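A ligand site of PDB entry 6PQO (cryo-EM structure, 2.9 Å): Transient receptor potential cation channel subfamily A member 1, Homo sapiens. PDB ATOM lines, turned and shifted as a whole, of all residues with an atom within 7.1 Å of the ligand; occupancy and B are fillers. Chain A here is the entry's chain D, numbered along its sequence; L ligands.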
ATOM      1  N   ASP A 607      15.717 -14.540 -14.904  1.00  0.00           N
ATOM      2  CA  ASP A 607      16.205 -13.440 -15.743  1.00  0.00           C
ATOM      3  C   ASP A 607      17.289 -12.653 -15.022  1.00  0.00           C
ATOM      4  O   ASP A 607      18.334 -12.363 -15.613  1.00  0.00           O
ATOM      5  CB  ASP A 607      15.042 -12.533 -16.126  1.00  0.00           C
ATOM      6  CG  ASP A 607      14.052 -13.222 -17.033  1.00  0.00           C
ATOM      7  OD1 ASP A 607      14.467 -14.095 -17.822  1.00  0.00           O
ATOM      8  OD2 ASP A 607      12.842 -12.899 -16.965  1.00  0.00           O
ATOM      9  N   LEU A 610      20.307 -14.519 -15.029  1.00  0.00           N
ATOM     10  CA  LEU A 610      20.968 -14.514 -16.321  1.00  0.00           C
ATOM     11  C   LEU A 610      21.803 -13.254 -16.519  1.00  0.00           C
ATOM     12  O   LEU A 610      22.693 -13.252 -17.375  1.00  0.00           O
ATOM     13  CB  LEU A 610      19.903 -14.644 -17.418  1.00  0.00           C
ATOM     14  CG  LEU A 610      20.324 -14.918 -18.854  1.00  0.00           C
ATOM     15  CD1 LEU A 610      21.011 -16.259 -18.923  1.00  0.00           C
ATOM     16  CD2 LEU A 610      19.118 -14.881 -19.770  1.00  0.00           C
ATOM     17  N   LYS A 611      21.565 -12.211 -15.719  1.00  0.00           N
ATOM     18  CA  LYS A 611      22.147 -10.908 -16.044  1.00  0.00           C
ATOM     19  C   LYS A 611      23.634 -10.832 -15.727  1.00  0.00           C
ATOM     20  O   LYS A 611      24.416 -10.339 -16.544  1.00  0.00           O
ATOM     21  CB  LYS A 611      21.398  -9.797 -15.298  1.00  0.00           C
ATOM     22  CG  LYS A 611      19.999  -9.555 -15.809  1.00  0.00           C
ATOM     23  CD  LYS A 611      19.323  -8.431 -15.036  1.00  0.00           C
ATOM     24  CE  LYS A 611      17.946  -8.145 -15.597  1.00  0.00           C
ATOM     25  NZ  LYS A 611      17.022  -9.282 -15.383  1.00  0.00           N
ATOM     26  N   PHE A 613      27.479 -11.770 -14.954  1.00  0.00           N
ATOM     27  CA  PHE A 613      28.677 -12.592 -15.114  1.00  0.00           C
ATOM     28  C   PHE A 613      29.824 -11.647 -15.439  1.00  0.00           C
ATOM     29  O   PHE A 613      29.663 -10.425 -15.423  1.00  0.00           O
ATOM     30  CB  PHE A 613      28.488 -13.676 -16.177  1.00  0.00           C
ATOM     31  CG  PHE A 613      28.198 -13.158 -17.564  1.00  0.00           C
ATOM     32  CD1 PHE A 613      26.910 -12.882 -17.954  1.00  0.00           C
ATOM     33  CD2 PHE A 613      29.233 -13.002 -18.482  1.00  0.00           C
ATOM     34  CE1 PHE A 613      26.641 -12.410 -19.227  1.00  0.00           C
ATOM     35  CE2 PHE A 613      28.964 -12.530 -19.755  1.00  0.00           C
ATOM     36  CZ  PHE A 613      27.669 -12.245 -20.127  1.00  0.00           C
ATOM     37  N   HIS A 615      32.844 -10.447 -18.122  1.00  0.00           N
ATOM     38  CA  HIS A 615      33.234 -10.467 -19.530  1.00  0.00           C
ATOM     39  C   HIS A 615      34.708 -10.760 -19.744  1.00  0.00           C
ATOM     40  O   HIS A 615      35.126 -10.913 -20.893  1.00  0.00           O
ATOM     41  CB  HIS A 615      32.891  -9.118 -20.181  1.00  0.00           C
ATOM     42  CG  HIS A 615      31.423  -8.823 -20.218  1.00  0.00           C
ATOM     43  ND1 HIS A 615      30.567  -9.428 -21.105  1.00  0.00           N
ATOM     44  CD2 HIS A 615      30.667  -7.986 -19.462  1.00  0.00           C
ATOM     45  CE1 HIS A 615      29.346  -8.970 -20.913  1.00  0.00           C
ATOM     46  NE2 HIS A 615      29.376  -8.096 -19.918  1.00  0.00           N
ATOM     47  N   LYS A 621      31.966 -17.908 -18.247  1.00  0.00           N
ATOM     48  CA  LYS A 621      31.461 -17.256 -19.450  1.00  0.00           C
ATOM     49  C   LYS A 621      29.964 -17.009 -19.317  1.00  0.00           C
ATOM     50  O   LYS A 621      29.413 -17.073 -18.223  1.00  0.00           O
ATOM     51  CB  LYS A 621      31.763 -18.102 -20.684  1.00  0.00           C
ATOM     52  CG  LYS A 621      33.237 -18.193 -21.005  1.00  0.00           C
ATOM     53  CD  LYS A 621      33.477 -18.932 -22.310  1.00  0.00           C
ATOM     54  CE  LYS A 621      33.258 -20.418 -22.153  1.00  0.00           C
ATOM     55  NZ  LYS A 621      33.601 -21.158 -23.397  1.00  0.00           N
ATOM     56  N   CYS A 622      29.327 -16.666 -20.440  1.00  0.00           N
ATOM     57  CA  CYS A 622      27.875 -16.513 -20.461  1.00  0.00           C
ATOM     58  C   CYS A 622      27.214 -17.842 -20.132  1.00  0.00           C
ATOM     59  O   CYS A 622      27.608 -18.881 -20.686  1.00  0.00           O
ATOM     60  CB  CYS A 622      27.425 -16.022 -21.842  1.00  0.00           C
ATOM     61  SG  CYS A 622      25.655 -15.775 -22.029  1.00  0.00           S
ATOM     62  N   PRO A 623      26.220 -17.869 -19.245  1.00  0.00           N
ATOM     63  CA  PRO A 623      25.705 -19.150 -18.743  1.00  0.00           C
ATOM     64  C   PRO A 623      24.912 -19.952 -19.756  1.00  0.00           C
ATOM     65  O   PRO A 623      24.724 -21.155 -19.546  1.00  0.00           O
ATOM     66  CB  PRO A 623      24.826 -18.735 -17.560  1.00  0.00           C
ATOM     67  CG  PRO A 623      24.438 -17.340 -17.845  1.00  0.00           C
ATOM     68  CD  PRO A 623      25.607 -16.726 -18.537  1.00  0.00           C
ATOM     69  N   ILE A 624      24.437 -19.342 -20.853  1.00  0.00           N
ATOM     70  CA  ILE A 624      23.745 -20.118 -21.867  1.00  0.00           C
ATOM     71  C   ILE A 624      24.718 -21.020 -22.610  1.00  0.00           C
ATOM     72  O   ILE A 624      24.446 -22.202 -22.852  1.00  0.00           O
ATOM     73  CB  ILE A 624      22.988 -19.184 -22.835  1.00  0.00           C
ATOM     74  CG1 ILE A 624      21.990 -18.341 -22.052  1.00  0.00           C
ATOM     75  CG2 ILE A 624      22.267 -19.983 -23.891  1.00  0.00           C
ATOM     76  CD1 ILE A 624      20.935 -19.157 -21.361  1.00  0.00           C
ATOM     77  N   THR A 625      25.901 -20.490 -22.945  1.00  0.00           N
ATOM     78  CA  THR A 625      26.946 -21.320 -23.532  1.00  0.00           C
ATOM     79  C   THR A 625      27.450 -22.361 -22.546  1.00  0.00           C
ATOM     80  O   THR A 625      27.827 -23.466 -22.957  1.00  0.00           O
ATOM     81  CB  THR A 625      28.108 -20.439 -23.994  1.00  0.00           C
ATOM     82  OG1 THR A 625      28.707 -19.814 -22.852  1.00  0.00           O
ATOM     83  CG2 THR A 625      27.600 -19.360 -24.922  1.00  0.00           C
ATOM     84  N   GLU A 626      27.418 -22.049 -21.254  1.00  0.00           N
ATOM     85  CA  GLU A 626      27.795 -23.023 -20.242  1.00  0.00           C
ATOM     86  C   GLU A 626      26.784 -24.157 -20.168  1.00  0.00           C
ATOM     87  O   GLU A 626      27.172 -25.328 -20.012  1.00  0.00           O
ATOM     88  CB  GLU A 626      27.912 -22.332 -18.890  1.00  0.00           C
ATOM     89  CG  GLU A 626      28.993 -21.270 -18.824  1.00  0.00           C
ATOM     90  CD  GLU A 626      30.380 -21.853 -18.934  1.00  0.00           C
ATOM     91  OE1 GLU A 626      30.598 -22.980 -18.455  1.00  0.00           O
ATOM     92  OE2 GLU A 626      31.265 -21.177 -19.506  1.00  0.00           O
ATOM     93  N   LYS A 662      14.380 -15.132 -27.686  1.00  0.00           N
ATOM     94  CA  LYS A 662      15.071 -14.184 -26.830  1.00  0.00           C
ATOM     95  C   LYS A 662      16.348 -14.752 -26.227  1.00  0.00           C
ATOM     96  O   LYS A 662      17.210 -13.968 -25.820  1.00  0.00           O
ATOM     97  CB  LYS A 662      14.139 -13.715 -25.714  1.00  0.00           C
ATOM     98  CG  LYS A 662      13.733 -14.773 -24.728  1.00  0.00           C
ATOM     99  CD  LYS A 662      12.762 -14.230 -23.699  1.00  0.00           C
ATOM    100  CE  LYS A 662      13.461 -13.268 -22.752  1.00  0.00           C
ATOM    101  NZ  LYS A 662      12.561 -12.828 -21.663  1.00  0.00           N
ATOM    102  N   TYR A 663      16.507 -16.075 -26.169  1.00  0.00           N
ATOM    103  CA  TYR A 663      17.681 -16.669 -25.556  1.00  0.00           C
ATOM    104  C   TYR A 663      18.719 -17.133 -26.560  1.00  0.00           C
ATOM    105  O   TYR A 663      19.799 -17.570 -26.154  1.00  0.00           O
ATOM    106  CB  TYR A 663      17.292 -17.856 -24.673  1.00  0.00           C
ATOM    107  CG  TYR A 663      16.448 -17.478 -23.485  1.00  0.00           C
ATOM    108  CD1 TYR A 663      17.004 -16.815 -22.409  1.00  0.00           C
ATOM    109  CD2 TYR A 663      15.112 -17.824 -23.434  1.00  0.00           C
ATOM    110  CE1 TYR A 663      16.235 -16.471 -21.313  1.00  0.00           C
ATOM    111  CE2 TYR A 663      14.341 -17.494 -22.347  1.00  0.00           C
ATOM    112  CZ  TYR A 663      14.902 -16.818 -21.292  1.00  0.00           C
ATOM    113  OH  TYR A 663      14.131 -16.488 -20.205  1.00  0.00           O
ATOM    114  N   LEU A 664      18.440 -17.058 -27.859  1.00  0.00           N
ATOM    115  CA  LEU A 664      19.314 -17.680 -28.833  1.00  0.00           C
ATOM    116  C   LEU A 664      20.443 -16.783 -29.299  1.00  0.00           C
ATOM    117  O   LEU A 664      21.369 -17.281 -29.951  1.00  0.00           O
ATOM    118  CB  LEU A 664      18.514 -18.143 -30.061  1.00  0.00           C
ATOM    119  CG  LEU A 664      17.824 -19.505 -30.006  1.00  0.00           C
ATOM    120  CD1 LEU A 664      16.590 -19.505 -29.134  1.00  0.00           C
ATOM    121  CD2 LEU A 664      17.462 -19.950 -31.392  1.00  0.00           C
ATOM    122  N   GLN A 665      20.431 -15.497 -28.968  1.00  0.00           N
ATOM    123  CA  GLN A 665      21.477 -14.617 -29.442  1.00  0.00           C
ATOM    124  C   GLN A 665      21.682 -13.473 -28.461  1.00  0.00           C
ATOM    125  O   GLN A 665      20.802 -13.122 -27.677  1.00  0.00           O
ATOM    126  CB  GLN A 665      21.160 -14.056 -30.823  1.00  0.00           C
ATOM    127  CG  GLN A 665      19.934 -13.164 -30.860  1.00  0.00           C
ATOM    128  CD  GLN A 665      19.625 -12.671 -32.258  1.00  0.00           C
ATOM    129  OE1 GLN A 665      20.368 -12.933 -33.199  1.00  0.00           O
ATOM    130  NE2 GLN A 665      18.523 -11.948 -32.386  1.00  0.00           N
ATOM    131  N   CYS A 666      22.887 -12.901 -28.514  1.00  0.00           N
ATOM    132  CA  CYS A 666      23.231 -11.727 -27.741  1.00  0.00           C
ATOM    133  C   CYS A 666      22.555 -10.509 -28.370  1.00  0.00           C
ATOM    134  O   CYS A 666      22.056 -10.577 -29.493  1.00  0.00           O
ATOM    135  CB  CYS A 666      24.741 -11.559 -27.697  1.00  0.00           C
ATOM    136  SG  CYS A 666      25.478 -11.184 -29.298  1.00  0.00           S
ATOM    137  N   PRO A 667      22.493  -9.379 -27.656  1.00  0.00           N
ATOM    138  CA  PRO A 667      22.128  -8.126 -28.315  1.00  0.00           C
ATOM    139  C   PRO A 667      23.153  -7.731 -29.365  1.00  0.00           C
ATOM    140  O   PRO A 667      24.348  -7.996 -29.235  1.00  0.00           O
ATOM    141  CB  PRO A 667      22.071  -7.114 -27.164  1.00  0.00           C
ATOM    142  CG  PRO A 667      21.751  -7.935 -25.987  1.00  0.00           C
ATOM    143  CD  PRO A 667      22.469  -9.234 -26.186  1.00  0.00           C
ATOM    144  N   PHE A 670      26.870  -5.857 -29.158  1.00  0.00           N
ATOM    145  CA  PHE A 670      28.084  -6.574 -28.837  1.00  0.00           C
ATOM    146  C   PHE A 670      28.661  -7.318 -30.028  1.00  0.00           C
ATOM    147  O   PHE A 670      29.791  -7.816 -29.946  1.00  0.00           O
ATOM    148  CB  PHE A 670      27.818  -7.554 -27.699  1.00  0.00           C
ATOM    149  CG  PHE A 670      27.473  -6.893 -26.402  1.00  0.00           C
ATOM    150  CD1 PHE A 670      28.466  -6.387 -25.578  1.00  0.00           C
ATOM    151  CD2 PHE A 670      26.142  -6.755 -26.017  1.00  0.00           C
ATOM    152  CE1 PHE A 670      28.145  -5.770 -24.387  1.00  0.00           C
ATOM    153  CE2 PHE A 670      25.821  -6.137 -24.826  1.00  0.00           C
ATOM    154  CZ  PHE A 670      26.825  -5.649 -24.011  1.00  0.00           C
ATOM    155  N   TYR A 681      31.258 -10.459 -29.584  1.00  0.00           N
ATOM    156  CA  TYR A 681      30.697 -11.796 -29.718  1.00  0.00           C
ATOM    157  C   TYR A 681      30.316 -12.013 -31.176  1.00  0.00           C
ATOM    158  O   TYR A 681      29.780 -11.112 -31.828  1.00  0.00           O
ATOM    159  CB  TYR A 681      29.469 -11.980 -28.828  1.00  0.00           C
ATOM    160  CG  TYR A 681      29.769 -11.918 -27.362  1.00  0.00           C
ATOM    161  CD1 TYR A 681      30.300 -13.021 -26.692  1.00  0.00           C
ATOM    162  CD2 TYR A 681      29.518 -10.772 -26.618  1.00  0.00           C
ATOM    163  CE1 TYR A 681      30.581 -12.971 -25.349  1.00  0.00           C
ATOM    164  CE2 TYR A 681      29.784 -10.719 -25.266  1.00  0.00           C
ATOM    165  CZ  TYR A 681      30.314 -11.814 -24.637  1.00  0.00           C
ATOM    166  OH  TYR A 681      30.587 -11.770 -23.293  1.00  0.00           O
ATOM    167  N   THR A 685      25.020 -16.763 -31.447  1.00  0.00           N
ATOM    168  CA  THR A 685      25.911 -17.203 -30.385  1.00  0.00           C
ATOM    169  C   THR A 685      25.590 -18.617 -29.939  1.00  0.00           C
ATOM    170  O   THR A 685      26.469 -19.500 -29.917  1.00  0.00           O
ATOM    171  CB  THR A 685      25.804 -16.266 -29.196  1.00  0.00           C
ATOM    172  OG1 THR A 685      24.488 -16.361 -28.650  1.00  0.00           O
ATOM    173  CG2 THR A 685      26.023 -14.842 -29.622  1.00  0.00           C
ATOM    174  N   ALA A 686      24.331 -18.860 -29.563  1.00  0.00           N
ATOM    175  CA  ALA A 686      23.922 -20.157 -29.060  1.00  0.00           C
ATOM    176  C   ALA A 686      24.022 -21.230 -30.134  1.00  0.00           C
ATOM    177  O   ALA A 686      24.357 -22.372 -29.834  1.00  0.00           O
ATOM    178  CB  ALA A 686      22.510 -20.099 -28.509  1.00  0.00           C
HETATM  179  C1  LIG L   1      24.348 -15.167 -24.607  1.00  0.00           C
HETATM  180  C2  LIG L   1      22.148 -14.458 -23.668  1.00  0.00           C
HETATM  181  C3  LIG L   1      21.072 -13.374 -24.000  1.00  0.00           C
HETATM  182  C4  LIG L   1      19.706 -13.542 -23.285  1.00  0.00           C
HETATM  183  C5  LIG L   1      19.205 -11.259 -22.831  1.00  0.00           C
HETATM  184  C6  LIG L   1      24.313 -12.962 -23.571  1.00  0.00           C
HETATM  185  C7  LIG L   1      24.750 -10.822 -22.787  1.00  0.00           C
HETATM  186  C8  LIG L   1      24.278  -9.433 -22.376  1.00  0.00           C
HETATM  187  C9  LIG L   1      22.960  -8.980 -22.576  1.00  0.00           C
HETATM  188  C10 LIG L   1      22.510  -7.685 -22.300  1.00  0.00           C
HETATM  189  C11 LIG L   1      23.376  -6.711 -21.789  1.00  0.00           C
HETATM  190  C12 LIG L   1      21.952  -5.259 -20.551  1.00  0.00           C
HETATM  191  C13 LIG L   1      24.703  -7.122 -21.580  1.00  0.00           C
HETATM  192  C14 LIG L   1      25.122  -8.425 -21.859  1.00  0.00           C
HETATM  193  C15 LIG L   1      25.843 -11.041 -23.565  1.00  0.00           C
HETATM  194  C16 LIG L   1      25.100 -16.106 -23.671  1.00  0.00           C
HETATM  195  N1  LIG L   1      23.585 -14.127 -24.021  1.00  0.00           N
HETATM  196  N2  LIG L   1      23.870 -11.966 -22.800  1.00  0.00           N
HETATM  197  O1  LIG L   1      24.214 -15.437 -25.767  1.00  0.00           O
HETATM  198  O2  LIG L   1      19.557 -12.511 -22.324  1.00  0.00           O
HETATM  199  O3  LIG L   1      22.972  -5.435 -21.508  1.00  0.00           O
HETATM  200  S1  LIG L   1      25.868 -12.578 -24.346  1.00  0.00           S
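The side-chain sulfur (SG) of Cys 622 is bonded to a carbon (C16) of the ligand (1.8 Å). The side-chain hydroxyl of Thr 685 sits at hydrogen-bond distance from an oxygen (O1) of the ligand, 3.0 Å away.
The side-chain hydroxyl (OG1) of Thr 625 is in hydrogen-bond range of the backbone carbonyl oxygen (O) of Cys 622. The backbone NH of Tyr 681 is in hydrogen-bond range of the backbone carbonyl oxygen of Phe 670 (3.0 Å).
Residues that only touch the ligand: Leu 610 (3.5 Å), Ile 624 (3.8 Å), Lys 662 (3.6 Å), Gln 665 (3.7 Å), Cys 666 (3.7 Å), Pro 667 (3.7 Å) and Phe 670 (3.5 Å). Hydrophobic or aromatic side chains that line the ligand: Leu 610, Ile 624, Pro 667 and Phe 670. Of the 21 residues printed, 9 come within 4 Å of the ligand. The nearest printed residue that does not touch the ligand is Phe 613 (4.1 Å).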
